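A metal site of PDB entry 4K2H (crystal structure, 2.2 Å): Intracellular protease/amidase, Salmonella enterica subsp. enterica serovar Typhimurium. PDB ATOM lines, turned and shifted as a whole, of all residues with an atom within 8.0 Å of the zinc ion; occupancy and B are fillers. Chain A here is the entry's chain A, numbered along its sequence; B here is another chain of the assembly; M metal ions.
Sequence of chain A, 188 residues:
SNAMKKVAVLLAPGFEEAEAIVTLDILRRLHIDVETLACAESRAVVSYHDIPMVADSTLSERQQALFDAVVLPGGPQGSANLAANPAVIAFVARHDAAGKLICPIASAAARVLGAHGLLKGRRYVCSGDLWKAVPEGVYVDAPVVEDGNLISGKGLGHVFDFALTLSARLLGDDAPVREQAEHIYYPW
The side-chain hydroxyl (OG) of Ser 47 is in hydrogen-bond range of the side-chain carboxylate (OE1) of Glu 17 (2.7 Å). The side-chain carboxylate (OE2) of Glu 16 sits at hydrogen-bond distance from the backbone NH (N) of Ala 18, at 2.8 Å. N of His 49 lies close to OG of Ser 47, at 3.4 Å. O of His 49 lies within hydrogen-bond range of NH1 of Arg 28 of chain B (2.8 Å). The side-chain carboxylate of Asp 25 of chain B lies within salt-bridge range of the guanidinium group of Arg 29 of chain B, at 2.9 Å. The guanidinium group (NH2) of Arg 29 of chain B lies close to the side-chain carboxylate (OE1) of Glu 16, at 3.5 Å.
Of the 20 residues printed, 4 come within 4 Å of the zinc ion. The nearest printed residue that does not touch the zinc ion is Ala 18 (4.3 Å).
The zinc ion is bound by the side-chain carboxylate of Glu 17 (1.8 Å), the side-chain carboxylate of Glu 16 (2.0 Å), the side-chain carboxylate of Asp 25 of chain B (2.0 Å) and a ring nitrogen (ND1) of His 49 (2.0 Å).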
ATOM      1  N   GLY A  14      15.245  -4.526 -30.402  1.00  0.00           N
ATOM      2  CA  GLY A  14      16.333  -3.594 -30.110  1.00  0.00           C
ATOM      3  C   GLY A  14      16.005  -2.358 -29.283  1.00  0.00           C
ATOM      4  O   GLY A  14      16.825  -1.511 -29.115  1.00  0.00           O
ATOM      5  N   PHE A  15      14.807  -2.273 -28.743  1.00  0.00           N
ATOM      6  CA  PHE A  15      14.414  -1.160 -27.883  1.00  0.00           C
ATOM      7  C   PHE A  15      15.357  -1.070 -26.712  1.00  0.00           C
ATOM      8  O   PHE A  15      15.794  -2.090 -26.218  1.00  0.00           O
ATOM      9  CB  PHE A  15      12.965  -1.336 -27.387  1.00  0.00           C
ATOM     10  CG  PHE A  15      12.761  -2.461 -26.371  1.00  0.00           C
ATOM     11  CD1 PHE A  15      12.702  -2.178 -25.016  1.00  0.00           C
ATOM     12  CD2 PHE A  15      12.593  -3.789 -26.766  1.00  0.00           C
ATOM     13  CE1 PHE A  15      12.480  -3.159 -24.073  1.00  0.00           C
ATOM     14  CE2 PHE A  15      12.392  -4.790 -25.838  1.00  0.00           C
ATOM     15  CZ  PHE A  15      12.300  -4.473 -24.482  1.00  0.00           C
ATOM     16  N   GLU A  16      15.650   0.158 -26.255  1.00  0.00           N
ATOM     17  CA  GLU A  16      16.525   0.376 -25.153  1.00  0.00           C
ATOM     18  C   GLU A  16      15.728   0.050 -23.904  1.00  0.00           C
ATOM     19  O   GLU A  16      14.805   0.784 -23.548  1.00  0.00           O
ATOM     20  CB  GLU A  16      17.037   1.824 -25.123  1.00  0.00           C
ATOM     21  CG  GLU A  16      18.495   1.954 -24.731  1.00  0.00           C
ATOM     22  CD  GLU A  16      18.888   1.006 -23.614  1.00  0.00           C
ATOM     23  OE1 GLU A  16      19.826   0.193 -23.828  1.00  0.00           O
ATOM     24  OE2 GLU A  16      18.222   1.040 -22.549  1.00  0.00           O
ATOM     25  N   GLU A  17      16.079  -1.055 -23.242  1.00  0.00           N
ATOM     26  CA  GLU A  17      15.294  -1.555 -22.137  1.00  0.00           C
ATOM     27  C   GLU A  17      15.325  -0.685 -20.913  1.00  0.00           C
ATOM     28  O   GLU A  17      14.339  -0.577 -20.202  1.00  0.00           O
ATOM     29  CB  GLU A  17      15.648  -2.993 -21.786  1.00  0.00           C
ATOM     30  CG  GLU A  17      17.019  -3.257 -21.164  1.00  0.00           C
ATOM     31  CD  GLU A  17      18.201  -2.870 -22.011  1.00  0.00           C
ATOM     32  OE1 GLU A  17      18.217  -3.277 -23.191  1.00  0.00           O
ATOM     33  OE2 GLU A  17      19.097  -2.134 -21.493  1.00  0.00           O
ATOM     34  N   ALA A  18      16.465  -0.071 -20.644  1.00  0.00           N
ATOM     35  CA  ALA A  18      16.584   0.741 -19.444  1.00  0.00           C
ATOM     36  C   ALA A  18      15.661   1.971 -19.548  1.00  0.00           C
ATOM     37  O   ALA A  18      14.945   2.309 -18.592  1.00  0.00           O
ATOM     38  CB  ALA A  18      18.035   1.113 -19.215  1.00  0.00           C
ATOM     39  N   GLU A  19      15.599   2.567 -20.736  1.00  0.00           N
ATOM     40  CA  GLU A  19      14.774   3.748 -20.970  1.00  0.00           C
ATOM     41  C   GLU A  19      13.301   3.427 -20.786  1.00  0.00           C
ATOM     42  O   GLU A  19      12.596   4.125 -20.057  1.00  0.00           O
ATOM     43  CB  GLU A  19      14.975   4.279 -22.386  1.00  0.00           C
ATOM     44  CG  GLU A  19      16.349   4.839 -22.655  1.00  0.00           C
ATOM     45  CD  GLU A  19      16.581   5.118 -24.139  1.00  0.00           C
ATOM     46  OE1 GLU A  19      15.635   5.054 -24.949  1.00  0.00           O
ATOM     47  OE2 GLU A  19      17.740   5.358 -24.484  1.00  0.00           O
ATOM     48  N   SER A  47      15.324  -6.778 -26.318  1.00  0.00           N
ATOM     49  CA  SER A  47      15.863  -5.422 -26.183  1.00  0.00           C
ATOM     50  C   SER A  47      17.282  -5.280 -26.734  1.00  0.00           C
ATOM     51  O   SER A  47      18.003  -6.279 -27.017  1.00  0.00           O
ATOM     52  CB  SER A  47      15.900  -5.031 -24.691  1.00  0.00           C
ATOM     53  OG  SER A  47      17.065  -5.589 -24.031  1.00  0.00           O
ATOM     54  N   TYR A  48      17.725  -4.015 -26.812  1.00  0.00           N
ATOM     55  CA  TYR A  48      19.085  -3.655 -27.219  1.00  0.00           C
ATOM     56  C   TYR A  48      20.149  -4.458 -26.480  1.00  0.00           C
ATOM     57  O   TYR A  48      21.066  -4.971 -27.075  1.00  0.00           O
ATOM     58  CB  TYR A  48      19.309  -2.164 -26.969  1.00  0.00           C
ATOM     59  CG  TYR A  48      20.662  -1.578 -27.330  1.00  0.00           C
ATOM     60  CD1 TYR A  48      21.466  -2.110 -28.356  1.00  0.00           C
ATOM     61  CD2 TYR A  48      21.108  -0.424 -26.686  1.00  0.00           C
ATOM     62  CE1 TYR A  48      22.685  -1.529 -28.683  1.00  0.00           C
ATOM     63  CE2 TYR A  48      22.298   0.167 -26.994  1.00  0.00           C
ATOM     64  CZ  TYR A  48      23.097  -0.380 -27.972  1.00  0.00           C
ATOM     65  OH  TYR A  48      24.284   0.251 -28.231  1.00  0.00           O
ATOM     66  N   HIS A  49      20.050  -4.500 -25.158  1.00  0.00           N
ATOM     67  CA  HIS A  49      20.979  -5.278 -24.328  1.00  0.00           C
ATOM     68  C   HIS A  49      20.490  -6.698 -24.015  1.00  0.00           C
ATOM     69  O   HIS A  49      20.770  -7.242 -22.963  1.00  0.00           O
ATOM     70  CB  HIS A  49      21.368  -4.469 -23.083  1.00  0.00           C
ATOM     71  CG  HIS A  49      22.213  -3.278 -23.412  1.00  0.00           C
ATOM     72  ND1 HIS A  49      21.793  -1.986 -23.217  1.00  0.00           N
ATOM     73  CD2 HIS A  49      23.441  -3.190 -23.997  1.00  0.00           C
ATOM     74  CE1 HIS A  49      22.708  -1.153 -23.690  1.00  0.00           C
ATOM     75  NE2 HIS A  49      23.724  -1.853 -24.134  1.00  0.00           N
ATOM     76  N   ASP A  50      19.797  -7.291 -24.976  1.00  0.00           N
ATOM     77  CA  ASP A  50      19.460  -8.701 -25.021  1.00  0.00           C
ATOM     78  C   ASP A  50      18.552  -9.232 -23.949  1.00  0.00           C
ATOM     79  O   ASP A  50      18.685 -10.373 -23.555  1.00  0.00           O
ATOM     80  CB  ASP A  50      20.720  -9.563 -25.029  1.00  0.00           C
ATOM     81  CG  ASP A  50      21.483  -9.420 -26.294  1.00  0.00           C
ATOM     82  OD1 ASP A  50      20.828  -9.370 -27.371  1.00  0.00           O
ATOM     83  OD2 ASP A  50      22.732  -9.365 -26.205  1.00  0.00           O
ATOM     84  N   ILE A  51      17.587  -8.454 -23.512  1.00  0.00           N
ATOM     85  CA  ILE A  51      16.613  -8.984 -22.575  1.00  0.00           C
ATOM     86  C   ILE A  51      15.335  -9.247 -23.301  1.00  0.00           C
ATOM     87  O   ILE A  51      14.804  -8.350 -23.920  1.00  0.00           O
ATOM     88  CB  ILE A  51      16.343  -8.037 -21.410  1.00  0.00           C
ATOM     89  CG1 ILE A  51      17.674  -7.752 -20.714  1.00  0.00           C
ATOM     90  CG2 ILE A  51      15.383  -8.740 -20.434  1.00  0.00           C
ATOM     91  CD1 ILE A  51      17.551  -6.656 -19.696  1.00  0.00           C
ATOM     92  N   GLY A  75      17.322   3.225 -28.434  1.00  0.00           N
ATOM     93  CA  GLY A  75      18.076   2.075 -28.935  1.00  0.00           C
ATOM     94  C   GLY A  75      18.323   2.180 -30.431  1.00  0.00           C
ATOM     95  O   GLY A  75      17.409   2.519 -31.189  1.00  0.00           O
ATOM     96  N   LEU A 156      19.341   8.128 -21.453  1.00  0.00           N
ATOM     97  CA  LEU A 156      19.151   7.269 -20.295  1.00  0.00           C
ATOM     98  C   LEU A 156      19.490   7.948 -18.979  1.00  0.00           C
ATOM     99  O   LEU A 156      18.775   7.778 -17.987  1.00  0.00           O
ATOM    100  CB  LEU A 156      19.900   5.948 -20.439  1.00  0.00           C
ATOM    101  CG  LEU A 156      19.833   4.956 -19.261  1.00  0.00           C
ATOM    102  CD1 LEU A 156      18.394   4.580 -18.958  1.00  0.00           C
ATOM    103  CD2 LEU A 156      20.709   3.721 -19.515  1.00  0.00           C
ATOM    104  N   ILE B  21      17.412  -3.985 -14.299  1.00  0.00           N
ATOM    105  CA  ILE B  21      17.627  -3.667 -15.713  1.00  0.00           C
ATOM    106  C   ILE B  21      18.635  -2.549 -15.904  1.00  0.00           C
ATOM    107  O   ILE B  21      19.502  -2.632 -16.790  1.00  0.00           O
ATOM    108  CB  ILE B  21      16.283  -3.402 -16.454  1.00  0.00           C
ATOM    109  CG1 ILE B  21      15.829  -4.674 -17.136  1.00  0.00           C
ATOM    110  CG2 ILE B  21      16.396  -2.353 -17.535  1.00  0.00           C
ATOM    111  CD1 ILE B  21      15.793  -5.848 -16.180  1.00  0.00           C
ATOM    112  N   VAL B  22      18.577  -1.520 -15.082  1.00  0.00           N
ATOM    113  CA  VAL B  22      19.513  -0.431 -15.246  1.00  0.00           C
ATOM    114  C   VAL B  22      20.907  -0.952 -14.940  1.00  0.00           C
ATOM    115  O   VAL B  22      21.836  -0.644 -15.647  1.00  0.00           O
ATOM    116  CB  VAL B  22      19.194   0.755 -14.339  1.00  0.00           C
ATOM    117  CG1 VAL B  22      20.245   1.833 -14.522  1.00  0.00           C
ATOM    118  CG2 VAL B  22      17.792   1.312 -14.661  1.00  0.00           C
ATOM    119  N   LEU B  24      22.037  -3.928 -15.116  1.00  0.00           N
ATOM    120  CA  LEU B  24      22.402  -4.772 -16.233  1.00  0.00           C
ATOM    121  C   LEU B  24      22.756  -3.960 -17.481  1.00  0.00           C
ATOM    122  O   LEU B  24      23.740  -4.244 -18.171  1.00  0.00           O
ATOM    123  CB  LEU B  24      21.233  -5.687 -16.522  1.00  0.00           C
ATOM    124  CG  LEU B  24      21.402  -6.707 -17.615  1.00  0.00           C
ATOM    125  CD1 LEU B  24      20.574  -7.930 -17.216  1.00  0.00           C
ATOM    126  CD2 LEU B  24      20.978  -6.132 -18.977  1.00  0.00           C
ATOM    127  N   ASP B  25      21.922  -2.990 -17.804  1.00  0.00           N
ATOM    128  CA  ASP B  25      22.216  -2.118 -18.964  1.00  0.00           C
ATOM    129  C   ASP B  25      23.613  -1.516 -18.872  1.00  0.00           C
ATOM    130  O   ASP B  25      24.336  -1.480 -19.857  1.00  0.00           O
ATOM    131  CB  ASP B  25      21.138  -1.017 -19.058  1.00  0.00           C
ATOM    132  CG  ASP B  25      21.549   0.151 -19.959  1.00  0.00           C
ATOM    133  OD1 ASP B  25      22.329   1.026 -19.502  1.00  0.00           O
ATOM    134  OD2 ASP B  25      21.078   0.211 -21.105  1.00  0.00           O
ATOM    135  N   ILE B  26      23.964  -1.022 -17.681  1.00  0.00           N
ATOM    136  CA  ILE B  26      25.247  -0.363 -17.446  1.00  0.00           C
ATOM    137  C   ILE B  26      26.429  -1.355 -17.592  1.00  0.00           C
ATOM    138  O   ILE B  26      27.416  -1.075 -18.279  1.00  0.00           O
ATOM    139  CB  ILE B  26      25.316   0.288 -16.034  1.00  0.00           C
ATOM    140  CG1 ILE B  26      24.280   1.417 -15.920  1.00  0.00           C
ATOM    141  CG2 ILE B  26      26.712   0.831 -15.756  1.00  0.00           C
ATOM    142  CD1 ILE B  26      24.460   2.520 -16.944  1.00  0.00           C
ATOM    143  N   ARG B  28      26.454  -4.057 -19.260  1.00  0.00           N
ATOM    144  CA  ARG B  28      26.547  -4.604 -20.633  1.00  0.00           C
ATOM    145  C   ARG B  28      27.049  -3.541 -21.602  1.00  0.00           C
ATOM    146  O   ARG B  28      27.717  -3.885 -22.574  1.00  0.00           O
ATOM    147  CB  ARG B  28      25.235  -5.209 -21.104  1.00  0.00           C
ATOM    148  CG  ARG B  28      24.950  -6.530 -20.455  1.00  0.00           C
ATOM    149  CD  ARG B  28      23.903  -7.326 -21.220  1.00  0.00           C
ATOM    150  NE  ARG B  28      23.883  -8.689 -20.738  1.00  0.00           N
ATOM    151  CZ  ARG B  28      22.823  -9.477 -20.688  1.00  0.00           C
ATOM    152  NH1 ARG B  28      21.630  -9.038 -21.054  1.00  0.00           N
ATOM    153  NH2 ARG B  28      22.960 -10.696 -20.199  1.00  0.00           N
ATOM    154  N   ARG B  29      26.777  -2.259 -21.332  1.00  0.00           N
ATOM    155  CA  ARG B  29      27.458  -1.174 -22.078  1.00  0.00           C
ATOM    156  C   ARG B  29      28.995  -1.264 -21.965  1.00  0.00           C
ATOM    157  O   ARG B  29      29.689  -0.864 -22.856  1.00  0.00           O
ATOM    158  CB  ARG B  29      27.041   0.214 -21.597  1.00  0.00           C
ATOM    159  CG  ARG B  29      25.669   0.659 -22.086  1.00  0.00           C
ATOM    160  CD  ARG B  29      25.293   1.975 -21.443  1.00  0.00           C
ATOM    161  NE  ARG B  29      23.873   2.176 -21.662  1.00  0.00           N
ATOM    162  CZ  ARG B  29      23.353   2.675 -22.777  1.00  0.00           C
ATOM    163  NH1 ARG B  29      24.143   3.101 -23.749  1.00  0.00           N
ATOM    164  NH2 ARG B  29      22.046   2.791 -22.897  1.00  0.00           N
HETATM  165 ZN    ZN M   1      20.220  -1.064 -22.371  1.00  0.00          ZN
